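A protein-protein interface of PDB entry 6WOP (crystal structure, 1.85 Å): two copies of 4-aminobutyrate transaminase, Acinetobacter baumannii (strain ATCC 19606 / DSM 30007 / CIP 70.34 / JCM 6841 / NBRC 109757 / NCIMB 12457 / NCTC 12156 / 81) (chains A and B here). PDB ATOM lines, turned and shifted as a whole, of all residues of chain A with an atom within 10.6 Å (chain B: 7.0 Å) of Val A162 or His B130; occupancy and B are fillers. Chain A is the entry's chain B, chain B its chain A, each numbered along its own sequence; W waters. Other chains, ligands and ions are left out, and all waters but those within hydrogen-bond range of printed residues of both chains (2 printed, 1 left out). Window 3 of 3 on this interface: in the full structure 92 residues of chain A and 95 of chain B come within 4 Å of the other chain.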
ATOM      1  N   SER A 143      14.225  -2.966  33.151  1.00  0.00           N
ATOM      2  CA  SER A 143      14.014  -4.402  33.056  1.00  0.00           C
ATOM      3  C   SER A 143      12.514  -4.668  32.839  1.00  0.00           C
ATOM      4  O   SER A 143      11.684  -3.753  32.900  1.00  0.00           O
ATOM      5  CB  SER A 143      14.528  -5.062  34.353  1.00  0.00           C
ATOM      6  OG  SER A 143      13.432  -5.240  35.240  1.00  0.00           O
ATOM      7  N   PHE A 144      12.129  -5.858  32.373  1.00  0.00           N
ATOM      8  CA  PHE A 144      10.693  -6.090  32.243  1.00  0.00           C
ATOM      9  C   PHE A 144      10.015  -6.007  33.608  1.00  0.00           C
ATOM     10  O   PHE A 144       8.952  -5.390  33.731  1.00  0.00           O
ATOM     11  CB  PHE A 144      10.412  -7.450  31.581  1.00  0.00           C
ATOM     12  CG  PHE A 144      10.446  -7.361  30.084  1.00  0.00           C
ATOM     13  CD1 PHE A 144       9.340  -6.861  29.374  1.00  0.00           C
ATOM     14  CD2 PHE A 144      11.597  -7.652  29.393  1.00  0.00           C
ATOM     15  CE1 PHE A 144       9.387  -6.747  27.960  1.00  0.00           C
ATOM     16  CE2 PHE A 144      11.621  -7.513  27.965  1.00  0.00           C
ATOM     17  CZ  PHE A 144      10.523  -7.056  27.271  1.00  0.00           C
ATOM     18  N   MET A 145      10.612  -6.623  34.654  1.00  0.00           N
ATOM     19  CA  MET A 145       9.969  -6.483  35.974  1.00  0.00           C
ATOM     20  C   MET A 145      10.030  -5.029  36.472  1.00  0.00           C
ATOM     21  O   MET A 145       9.063  -4.535  37.062  1.00  0.00           O
ATOM     22  CB  MET A 145      10.599  -7.413  37.014  1.00  0.00           C
ATOM     23  CG  MET A 145       9.945  -7.341  38.429  1.00  0.00           C
ATOM     24  SD  MET A 145       8.135  -7.060  38.213  1.00  0.00           S
ATOM     25  CE  MET A 145       7.534  -8.726  38.070  1.00  0.00           C
ATOM     26  N   THR A 146      11.188  -4.354  36.336  1.00  0.00           N
ATOM     27  CA  THR A 146      11.241  -3.023  36.900  1.00  0.00           C
ATOM     28  C   THR A 146      10.491  -2.017  36.029  1.00  0.00           C
ATOM     29  O   THR A 146      10.009  -0.999  36.551  1.00  0.00           O
ATOM     30  CB  THR A 146      12.728  -2.600  37.168  1.00  0.00           C
ATOM     31  OG1 THR A 146      13.532  -2.792  35.996  1.00  0.00           O
ATOM     32  CG2 THR A 146      13.310  -3.454  38.262  1.00  0.00           C
ATOM     33  N   MET A 147      10.338  -2.274  34.721  1.00  0.00           N
ATOM     34  CA  MET A 147       9.409  -1.462  33.932  1.00  0.00           C
ATOM     35  C   MET A 147       7.981  -1.618  34.438  1.00  0.00           C
ATOM     36  O   MET A 147       7.214  -0.637  34.495  1.00  0.00           O
ATOM     37  CB  MET A 147       9.428  -1.887  32.435  1.00  0.00           C
ATOM     38  CG  MET A 147      10.615  -1.288  31.671  1.00  0.00           C
ATOM     39  SD  MET A 147      10.335  -1.725  29.852  1.00  0.00           S
ATOM     40  CE  MET A 147      10.806  -3.446  29.773  1.00  0.00           C
ATOM     41  N   ALA A 148       7.579  -2.847  34.711  1.00  0.00           N
ATOM     42  CA  ALA A 148       6.212  -3.054  35.217  1.00  0.00           C
ATOM     43  C   ALA A 148       6.033  -2.300  36.533  1.00  0.00           C
ATOM     44  O   ALA A 148       5.019  -1.606  36.751  1.00  0.00           O
ATOM     45  CB  ALA A 148       5.928  -4.573  35.408  1.00  0.00           C
ATOM     46  N   MET A 149       7.044  -2.380  37.413  1.00  0.00           N
ATOM     47  CA  MET A 149       6.975  -1.661  38.683  1.00  0.00           C
ATOM     48  C   MET A 149       6.945  -0.164  38.473  1.00  0.00           C
ATOM     49  O   MET A 149       6.204   0.549  39.173  1.00  0.00           O
ATOM     50  CB  MET A 149       8.157  -2.057  39.561  1.00  0.00           C
ATOM     51  CG  MET A 149       8.099  -3.545  39.922  1.00  0.00           C
ATOM     52  SD  MET A 149       9.678  -4.041  40.734  1.00  0.00           S
ATOM     53  CE  MET A 149       9.658  -2.961  42.169  1.00  0.00           C
ATOM     54  N   TYR A 156       8.762   4.875  28.893  1.00  0.00           N
ATOM     55  CA  TYR A 156       9.578   3.752  29.351  1.00  0.00           C
ATOM     56  C   TYR A 156       9.042   2.383  28.933  1.00  0.00           C
ATOM     57  O   TYR A 156       9.827   1.443  28.754  1.00  0.00           O
ATOM     58  CB  TYR A 156       9.680   3.747  30.873  1.00  0.00           C
ATOM     59  CG  TYR A 156      10.233   5.026  31.374  1.00  0.00           C
ATOM     60  CD1 TYR A 156      11.470   5.517  30.895  1.00  0.00           C
ATOM     61  CD2 TYR A 156       9.518   5.800  32.304  1.00  0.00           C
ATOM     62  CE1 TYR A 156      11.980   6.734  31.357  1.00  0.00           C
ATOM     63  CE2 TYR A 156      10.042   6.992  32.778  1.00  0.00           C
ATOM     64  CZ  TYR A 156      11.260   7.446  32.301  1.00  0.00           C
ATOM     65  OH  TYR A 156      11.730   8.636  32.762  1.00  0.00           O
ATOM     66  N   LYS A 157       7.732   2.176  28.901  1.00  0.00           N
ATOM     67  CA  LYS A 157       7.304   0.817  28.573  1.00  0.00           C
ATOM     68  C   LYS A 157       6.285   0.699  27.471  1.00  0.00           C
ATOM     69  O   LYS A 157       5.996  -0.437  27.088  1.00  0.00           O
ATOM     70  CB  LYS A 157       6.794   0.060  29.817  1.00  0.00           C
ATOM     71  CG  LYS A 157       5.905   0.851  30.715  1.00  0.00           C
ATOM     72  CD  LYS A 157       5.309  -0.047  31.881  1.00  0.00           C
ATOM     73  CE  LYS A 157       4.673   0.803  32.927  1.00  0.00           C
ATOM     74  NZ  LYS A 157       4.363  -0.013  34.150  1.00  0.00           N
ATOM     75  N   ARG A 158       5.826   1.807  26.881  1.00  0.00           N
ATOM     76  CA  ARG A 158       4.761   1.747  25.885  1.00  0.00           C
ATOM     77  C   ARG A 158       5.162   0.985  24.622  1.00  0.00           C
ATOM     78  O   ARG A 158       4.266   0.534  23.890  1.00  0.00           O
ATOM     79  CB  ARG A 158       4.338   3.157  25.481  1.00  0.00           C
ATOM     80  CG  ARG A 158       5.558   3.897  24.891  1.00  0.00           C
ATOM     81  CD  ARG A 158       5.204   5.135  24.140  1.00  0.00           C
ATOM     82  NE  ARG A 158       6.272   6.127  24.282  1.00  0.00           N
ATOM     83  CZ  ARG A 158       6.079   7.434  24.160  1.00  0.00           C
ATOM     84  NH1 ARG A 158       4.879   7.892  23.856  1.00  0.00           N
ATOM     85  NH2 ARG A 158       7.085   8.277  24.317  1.00  0.00           N
ATOM     86  N   ASP A 159       6.456   0.820  24.350  1.00  0.00           N
ATOM     87  CA  ASP A 159       6.929   0.106  23.154  1.00  0.00           C
ATOM     88  C   ASP A 159       7.025  -1.424  23.331  1.00  0.00           C
ATOM     89  O   ASP A 159       7.263  -2.119  22.333  1.00  0.00           O
ATOM     90  CB  ASP A 159       8.354   0.590  22.736  1.00  0.00           C
ATOM     91  CG  ASP A 159       8.394   2.019  22.268  1.00  0.00           C
ATOM     92  OD1 ASP A 159       7.380   2.479  21.744  1.00  0.00           O
ATOM     93  OD2 ASP A 159       9.486   2.678  22.466  1.00  0.00           O
ATOM     94  N   PHE A 160       6.938  -1.959  24.559  1.00  0.00           N
ATOM     95  CA  PHE A 160       7.422  -3.290  24.867  1.00  0.00           C
ATOM     96  C   PHE A 160       6.345  -4.284  25.311  1.00  0.00           C
ATOM     97  O   PHE A 160       6.700  -5.395  25.720  1.00  0.00           O
ATOM     98  CB  PHE A 160       8.528  -3.202  25.924  1.00  0.00           C
ATOM     99  CG  PHE A 160       9.643  -2.277  25.488  1.00  0.00           C
ATOM    100  CD1 PHE A 160      10.222  -2.475  24.235  1.00  0.00           C
ATOM    101  CD2 PHE A 160      10.019  -1.187  26.247  1.00  0.00           C
ATOM    102  CE1 PHE A 160      11.207  -1.604  23.746  1.00  0.00           C
ATOM    103  CE2 PHE A 160      11.030  -0.308  25.790  1.00  0.00           C
ATOM    104  CZ  PHE A 160      11.604  -0.546  24.546  1.00  0.00           C
ATOM    105  N   GLY A 161       5.056  -3.984  25.128  1.00  0.00           N
ATOM    106  CA  GLY A 161       4.106  -5.111  25.172  1.00  0.00           C
ATOM    107  C   GLY A 161       3.768  -5.556  26.588  1.00  0.00           C
ATOM    108  O   GLY A 161       3.840  -4.784  27.567  1.00  0.00           O
ATOM    109  N   VAL A 162       3.305  -6.825  26.686  1.00  0.00           N
ATOM    110  CA  VAL A 162       2.721  -7.306  27.938  1.00  0.00           C
ATOM    111  C   VAL A 162       3.741  -7.238  29.065  1.00  0.00           C
ATOM    112  O   VAL A 162       4.925  -7.586  28.886  1.00  0.00           O
ATOM    113  CB  VAL A 162       2.198  -8.747  27.739  1.00  0.00           C
ATOM    114  CG1 VAL A 162       3.304  -9.679  27.267  1.00  0.00           C
ATOM    115  CG2 VAL A 162       1.587  -9.328  29.102  1.00  0.00           C
ATOM    116  N   MET A 163       3.279  -6.827  30.276  1.00  0.00           N
ATOM    117  CA  MET A 163       4.180  -6.750  31.433  1.00  0.00           C
ATOM    118  C   MET A 163       3.969  -7.947  32.386  1.00  0.00           C
ATOM    119  O   MET A 163       2.956  -8.634  32.320  1.00  0.00           O
ATOM    120  CB  MET A 163       3.958  -5.422  32.182  1.00  0.00           C
ATOM    121  CG  MET A 163       4.394  -4.202  31.375  1.00  0.00           C
ATOM    122  SD  MET A 163       6.231  -4.190  31.322  1.00  0.00           S
ATOM    123  CE  MET A 163       6.602  -4.050  29.616  1.00  0.00           C
ATOM    124  N   PRO A 164       4.934  -8.254  33.261  1.00  0.00           N
ATOM    125  CA  PRO A 164       4.768  -9.397  34.166  1.00  0.00           C
ATOM    126  C   PRO A 164       3.543  -9.266  35.060  1.00  0.00           C
ATOM    127  O   PRO A 164       3.225  -8.196  35.577  1.00  0.00           O
ATOM    128  CB  PRO A 164       6.068  -9.392  34.991  1.00  0.00           C
ATOM    129  CG  PRO A 164       7.083  -8.745  34.095  1.00  0.00           C
ATOM    130  CD  PRO A 164       6.324  -7.739  33.230  1.00  0.00           C
ATOM    131  N   ALA A 165       2.906 -10.406  35.307  1.00  0.00           N
ATOM    132  CA  ALA A 165       1.710 -10.459  36.156  1.00  0.00           C
ATOM    133  C   ALA A 165       2.054 -10.128  37.602  1.00  0.00           C
ATOM    134  O   ALA A 165       3.166 -10.362  38.059  1.00  0.00           O
ATOM    135  CB  ALA A 165       1.089 -11.859  36.126  1.00  0.00           C
ATOM    136  N   GLY A 166       1.032  -9.665  38.349  1.00  0.00           N
ATOM    137  CA  GLY A 166       1.139  -9.511  39.791  1.00  0.00           C
ATOM    138  C   GLY A 166       1.809  -8.218  40.214  1.00  0.00           C
ATOM    139  O   GLY A 166       2.290  -8.133  41.325  1.00  0.00           O
ATOM    140  N   VAL A 167       1.859  -7.198  39.366  1.00  0.00           N
ATOM    141  CA  VAL A 167       2.399  -5.904  39.757  1.00  0.00           C
ATOM    142  C   VAL A 167       1.255  -4.914  39.617  1.00  0.00           C
ATOM    143  O   VAL A 167       0.603  -4.861  38.545  1.00  0.00           O
ATOM    144  CB  VAL A 167       3.593  -5.500  38.876  1.00  0.00           C
ATOM    145  CG1 VAL A 167       4.177  -4.139  39.339  1.00  0.00           C
ATOM    146  CG2 VAL A 167       4.665  -6.612  38.938  1.00  0.00           C
ATOM    147  N   VAL B 120      15.565  -8.353  23.651  1.00  0.00           N
ATOM    148  CA  VAL B 120      14.168  -8.809  23.681  1.00  0.00           C
ATOM    149  C   VAL B 120      13.205  -7.620  23.566  1.00  0.00           C
ATOM    150  O   VAL B 120      12.179  -7.698  22.852  1.00  0.00           O
ATOM    151  CB  VAL B 120      13.921  -9.625  24.975  1.00  0.00           C
ATOM    152  CG1 VAL B 120      12.375  -9.793  25.253  1.00  0.00           C
ATOM    153  CG2 VAL B 120      14.626 -11.020  24.866  1.00  0.00           C
ATOM    154  N   ALA B 123      13.267  -6.545  19.944  1.00  0.00           N
ATOM    155  CA  ALA B 123      12.548  -7.509  19.101  1.00  0.00           C
ATOM    156  C   ALA B 123      11.044  -7.428  19.312  1.00  0.00           C
ATOM    157  O   ALA B 123      10.273  -7.520  18.351  1.00  0.00           O
ATOM    158  CB  ALA B 123      13.024  -8.921  19.412  1.00  0.00           C
ATOM    159  N   ARG B 124      10.608  -7.313  20.565  1.00  0.00           N
ATOM    160  CA  ARG B 124       9.182  -7.165  20.827  1.00  0.00           C
ATOM    161  C   ARG B 124       8.669  -5.914  20.146  1.00  0.00           C
ATOM    162  O   ARG B 124       7.621  -5.935  19.514  1.00  0.00           O
ATOM    163  CB  ARG B 124       8.902  -7.063  22.308  1.00  0.00           C
ATOM    164  CG  ARG B 124       8.878  -8.403  23.067  1.00  0.00           C
ATOM    165  CD  ARG B 124       8.025  -8.204  24.303  1.00  0.00           C
ATOM    166  NE  ARG B 124       7.822  -9.384  25.165  1.00  0.00           N
ATOM    167  CZ  ARG B 124       7.073  -9.304  26.275  1.00  0.00           C
ATOM    168  NH1 ARG B 124       6.500  -8.145  26.589  1.00  0.00           N
ATOM    169  NH2 ARG B 124       6.904 -10.358  27.065  1.00  0.00           N
ATOM    170  N   THR B 127       8.668  -6.336  16.126  1.00  0.00           N
ATOM    171  CA  THR B 127       7.688  -7.276  15.613  1.00  0.00           C
ATOM    172  C   THR B 127       6.284  -6.987  16.118  1.00  0.00           C
ATOM    173  O   THR B 127       5.292  -7.471  15.526  1.00  0.00           O
ATOM    174  CB  THR B 127       8.090  -8.720  15.981  1.00  0.00           C
ATOM    175  OG1 THR B 127       8.065  -8.867  17.406  1.00  0.00           O
ATOM    176  CG2 THR B 127       9.548  -9.108  15.521  1.00  0.00           C
ATOM    177  N   GLY B 128       6.141  -6.215  17.187  1.00  0.00           N
ATOM    178  CA  GLY B 128       4.848  -6.087  17.821  1.00  0.00           C
ATOM    179  C   GLY B 128       4.328  -7.373  18.413  1.00  0.00           C
ATOM    180  O   GLY B 128       3.118  -7.506  18.603  1.00  0.00           O
ATOM    181  N   ARG B 129       5.213  -8.319  18.729  1.00  0.00           N
ATOM    182  CA  ARG B 129       4.895  -9.604  19.318  1.00  0.00           C
ATOM    183  C   ARG B 129       5.545  -9.740  20.678  1.00  0.00           C
ATOM    184  O   ARG B 129       6.439  -8.967  21.011  1.00  0.00           O
ATOM    185  CB  ARG B 129       5.363 -10.750  18.408  1.00  0.00           C
ATOM    186  CG  ARG B 129       4.940 -10.513  16.961  1.00  0.00           C
ATOM    187  CD  ARG B 129       5.704 -11.587  16.124  1.00  0.00           C
ATOM    188  NE  ARG B 129       5.272 -11.497  14.730  1.00  0.00           N
ATOM    189  CZ  ARG B 129       5.642 -12.328  13.776  1.00  0.00           C
ATOM    190  NH1 ARG B 129       6.494 -13.302  14.056  1.00  0.00           N
ATOM    191  NH2 ARG B 129       5.142 -12.184  12.534  1.00  0.00           N
ATOM    192  N   HIS B 130       5.082 -10.729  21.480  1.00  0.00           N
ATOM    193  CA  HIS B 130       5.584 -10.829  22.847  1.00  0.00           C
ATOM    194  C   HIS B 130       6.409 -12.061  23.109  1.00  0.00           C
ATOM    195  O   HIS B 130       7.191 -12.063  24.079  1.00  0.00           O
ATOM    196  CB  HIS B 130       4.407 -10.816  23.873  1.00  0.00           C
ATOM    197  CG  HIS B 130       3.716 -12.152  24.021  1.00  0.00           C
ATOM    198  ND1 HIS B 130       2.829 -12.651  23.083  1.00  0.00           N
ATOM    199  CD2 HIS B 130       3.805 -13.098  24.990  1.00  0.00           C
ATOM    200  CE1 HIS B 130       2.409 -13.851  23.471  1.00  0.00           C
ATOM    201  NE2 HIS B 130       2.979 -14.135  24.629  1.00  0.00           N
ATOM    202  N   GLY B 131       6.269 -13.121  22.308  1.00  0.00           N
ATOM    203  CA  GLY B 131       6.811 -14.400  22.745  1.00  0.00           C
ATOM    204  C   GLY B 131       8.301 -14.531  22.494  1.00  0.00           C
ATOM    205  O   GLY B 131       8.846 -13.959  21.539  1.00  0.00           O
ATOM    206  N   ILE B 132       8.944 -15.395  23.293  1.00  0.00           N
ATOM    207  CA  ILE B 132      10.378 -15.630  23.181  1.00  0.00           C
ATOM    208  C   ILE B 132      10.641 -17.118  23.305  1.00  0.00           C
ATOM    209  O   ILE B 132      10.166 -17.748  24.252  1.00  0.00           O
ATOM    210  CB  ILE B 132      11.114 -14.856  24.286  1.00  0.00           C
ATOM    211  CG1 ILE B 132      10.873 -13.335  24.162  1.00  0.00           C
ATOM    212  CG2 ILE B 132      12.619 -15.173  24.325  1.00  0.00           C
ATOM    213  CD1 ILE B 132      11.706 -12.731  22.940  1.00  0.00           C
ATOM    214  N   MET B 145      12.951 -11.590  33.544  1.00  0.00           N
ATOM    215  CA  MET B 145      12.799 -12.077  32.174  1.00  0.00           C
ATOM    216  C   MET B 145      13.965 -12.979  31.756  1.00  0.00           C
ATOM    217  O   MET B 145      13.748 -13.989  31.058  1.00  0.00           O
ATOM    218  CB  MET B 145      12.668 -10.922  31.186  1.00  0.00           C
ATOM    219  CG  MET B 145      12.473 -11.341  29.726  1.00  0.00           C
ATOM    220  SD  MET B 145      11.212 -12.700  29.533  1.00  0.00           S
ATOM    221  CE  MET B 145       9.812 -11.931  28.816  1.00  0.00           C
ATOM    222  N   PRO B 164       7.638 -14.668  33.955  1.00  0.00           N
ATOM    223  CA  PRO B 164       6.754 -14.021  32.973  1.00  0.00           C
ATOM    224  C   PRO B 164       6.273 -14.949  31.865  1.00  0.00           C
ATOM    225  O   PRO B 164       6.977 -15.842  31.388  1.00  0.00           O
ATOM    226  CB  PRO B 164       7.604 -12.863  32.417  1.00  0.00           C
ATOM    227  CG  PRO B 164       8.991 -13.112  32.903  1.00  0.00           C
ATOM    228  CD  PRO B 164       8.915 -13.921  34.136  1.00  0.00           C
ATOM    229  N   ALA B 165       5.051 -14.688  31.429  1.00  0.00           N
ATOM    230  CA  ALA B 165       4.410 -15.461  30.382  1.00  0.00           C
ATOM    231  C   ALA B 165       5.114 -15.290  29.039  1.00  0.00           C
ATOM    232  O   ALA B 165       5.769 -14.273  28.787  1.00  0.00           O
ATOM    233  CB  ALA B 165       2.957 -15.009  30.228  1.00  0.00           C
ATOM    234  N   GLY B 166       4.876 -16.264  28.138  1.00  0.00           N
ATOM    235  CA  GLY B 166       5.318 -16.164  26.745  1.00  0.00           C
ATOM    236  C   GLY B 166       6.772 -16.550  26.506  1.00  0.00           C
ATOM    237  O   GLY B 166       7.352 -16.172  25.483  1.00  0.00           O
ATOM    238  N   VAL B 167       7.391 -17.274  27.434  1.00  0.00           N
ATOM    239  CA  VAL B 167       8.759 -17.776  27.252  1.00  0.00           C
ATOM    240  C   VAL B 167       8.724 -19.292  27.251  1.00  0.00           C
ATOM    241  O   VAL B 167       8.201 -19.892  28.203  1.00  0.00           O
ATOM    242  CB  VAL B 167       9.667 -17.273  28.381  1.00  0.00           C
ATOM    243  CG1 VAL B 167      11.157 -17.814  28.220  1.00  0.00           C
ATOM    244  CG2 VAL B 167       9.611 -15.736  28.380  1.00  0.00           C
ATOM    245  N   PHE B 168       9.327 -19.928  26.225  1.00  0.00           N
ATOM    246  CA  PHE B 168       9.275 -21.384  26.156  1.00  0.00           C
ATOM    247  C   PHE B 168      10.639 -21.930  25.779  1.00  0.00           C
ATOM    248  O   PHE B 168      11.379 -21.280  25.053  1.00  0.00           O
ATOM    249  CB  PHE B 168       8.166 -21.822  25.108  1.00  0.00           C
ATOM    250  CG  PHE B 168       6.791 -21.349  25.541  1.00  0.00           C
ATOM    251  CD1 PHE B 168       6.126 -21.997  26.601  1.00  0.00           C
ATOM    252  CD2 PHE B 168       6.213 -20.236  24.952  1.00  0.00           C
ATOM    253  CE1 PHE B 168       4.851 -21.499  27.052  1.00  0.00           C
ATOM    254  CE2 PHE B 168       4.986 -19.753  25.385  1.00  0.00           C
ATOM    255  CZ  PHE B 168       4.313 -20.388  26.431  1.00  0.00           C
ATOM    256  N   ILE B 196       2.469 -21.529  21.498  1.00  0.00           N
ATOM    257  CA  ILE B 196       2.391 -20.135  21.056  1.00  0.00           C
ATOM    258  C   ILE B 196       2.462 -20.091  19.533  1.00  0.00           C
ATOM    259  O   ILE B 196       3.366 -20.683  18.921  1.00  0.00           O
ATOM    260  CB  ILE B 196       3.502 -19.253  21.673  1.00  0.00           C
ATOM    261  CG1 ILE B 196       3.271 -17.803  21.223  1.00  0.00           C
ATOM    262  CG2 ILE B 196       4.988 -19.805  21.337  1.00  0.00           C
ATOM    263  CD1 ILE B 196       4.188 -16.747  21.935  1.00  0.00           C
ATOM    264  N   HIS B 199       3.120 -16.279  14.824  1.00  0.00           N
ATOM    265  CA  HIS B 199       2.989 -14.836  14.652  1.00  0.00           C
ATOM    266  C   HIS B 199       2.831 -14.124  15.990  1.00  0.00           C
ATOM    267  O   HIS B 199       2.656 -12.892  16.022  1.00  0.00           O
ATOM    268  CB  HIS B 199       1.817 -14.534  13.668  1.00  0.00           C
ATOM    269  CG  HIS B 199       2.127 -14.881  12.237  1.00  0.00           C
ATOM    270  ND1 HIS B 199       1.160 -14.977  11.254  1.00  0.00           N
ATOM    271  CD2 HIS B 199       3.310 -15.135  11.621  1.00  0.00           C
ATOM    272  CE1 HIS B 199       1.731 -15.272  10.100  1.00  0.00           C
ATOM    273  NE2 HIS B 199       3.035 -15.374  10.296  1.00  0.00           N
ATOM    274  N   ASP B 200       2.907 -14.854  17.102  1.00  0.00           N
ATOM    275  CA  ASP B 200       3.057 -14.187  18.393  1.00  0.00           C
ATOM    276  C   ASP B 200       4.464 -14.294  18.956  1.00  0.00           C
ATOM    277  O   ASP B 200       4.662 -13.956  20.131  1.00  0.00           O
ATOM    278  CB  ASP B 200       2.085 -14.767  19.411  1.00  0.00           C
ATOM    279  CG  ASP B 200       0.700 -14.222  19.236  1.00  0.00           C
ATOM    280  OD1 ASP B 200       0.565 -12.987  19.225  1.00  0.00           O
ATOM    281  OD2 ASP B 200      -0.233 -15.032  19.089  1.00  0.00           O
ATOM    282  N   VAL B 201       5.410 -14.861  18.208  1.00  0.00           N
ATOM    283  CA  VAL B 201       6.794 -15.027  18.691  1.00  0.00           C
ATOM    284  C   VAL B 201       7.615 -13.861  18.147  1.00  0.00           C
ATOM    285  O   VAL B 201       7.751 -13.716  16.932  1.00  0.00           O
ATOM    286  CB  VAL B 201       7.411 -16.384  18.262  1.00  0.00           C
ATOM    287  CG1 VAL B 201       8.882 -16.530  18.711  1.00  0.00           C
ATOM    288  CG2 VAL B 201       6.596 -17.575  18.803  1.00  0.00           C
ATOM    289  N   ALA B 202       8.206 -13.057  19.057  1.00  0.00           N
ATOM    290  CA  ALA B 202       9.080 -11.948  18.666  1.00  0.00           C
ATOM    291  C   ALA B 202      10.463 -12.433  18.263  1.00  0.00           C
ATOM    292  O   ALA B 202      11.038 -11.933  17.285  1.00  0.00           O
ATOM    293  CB  ALA B 202       9.236 -10.920  19.811  1.00  0.00           C
ATOM    294  N   ALA B 203      11.040 -13.370  19.010  1.00  0.00           N
ATOM    295  CA  ALA B 203      12.407 -13.755  18.727  1.00  0.00           C
ATOM    296  C   ALA B 203      12.644 -15.171  19.184  1.00  0.00           C
ATOM    297  O   ALA B 203      12.039 -15.640  20.167  1.00  0.00           O
ATOM    298  CB  ALA B 203      13.439 -12.844  19.438  1.00  0.00           C
HETATM  299  O   HOH W   1       3.209 -12.866  33.266  1.00  0.00           O
HETATM  300  O   HOH W   2      10.385  -9.846  33.809  1.00  0.00           O
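The guanidinium group (NH1) of Arg B124 sits at hydrogen-bond distance from the backbone carbonyl oxygen (O) of Phe A160. The backbone carbonyl oxygen (O) of Val A162 lies within hydrogen-bond range of the guanidinium group (NH1) of Arg B124 (2.8 Å).
The backbone carbonyl oxygen (O) of Arg B124 sits at hydrogen-bond distance from the backbone NH (N) of Arg B129, at 3.5 Å. The guanidinium group of Arg B124 is in hydrogen-bond range of the backbone carbonyl oxygen of His B130, 3.0 Å away.
CE2 of Phe A144 touches CG1 of Val B120, at 3.6 Å. Arg B124 touches Phe A144. Phe A144 touches Met B145. Gly A161 touches Arg B124. His B130 touches Val A162.
Of chain A, only Val A162 (3.7 Å) comes within 4 Å of His B130. No residue of chain A comes within 4 Å of Gly B128. Gly B131 touches none of the printed residues of chain A. Ile B132 touches none of the printed residues of chain A. Printed residues of chain B within 4 Å of Phe A160: Arg B124. Of the printed residues of chain A, Val B120 touches Phe A144 (3.6 Å). Lys A157 touches none of the printed residues of chain B. Met A147 touches none of the printed residues of chain B. The nearest residue of chain A that does not touch His B130 is Gly A161 (5.9 Å). The nearest printed residue of chain B that does not touch Phe A160 is Val B120 (5.7 Å).
Printed residues of chain A that touch a printed residue of chain B: Phe A144, Phe A160, Gly A161 and Val A162. Of the 21 printed residues of chain B, 4 touch a printed residue of chain A. Printed residues of chain B that touch a printed residue of chain A: Val B120, Arg B124, His B130 and Met B145. Hydrophobic or aromatic side chains of chain B that line the printed part of chain A: Val B120, His B130 and Met B145. Among the printed residues, 7 pairs touch across the chains. Among the printed residues, no Asp or Glu carboxylate lies within 4 Å of a Lys or Arg side-chain nitrogen of the other chain.
5 positions are printed for both chains.
Water W2 lies within hydrogen-bond range of the backbone NH of Met B145 (3.1 Å) and the backbone NH of Met A145 (3.3 Å). Water W1 lies within hydrogen-bond range of the backbone NH of Ala B165 and the backbone NH of Ala A165.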
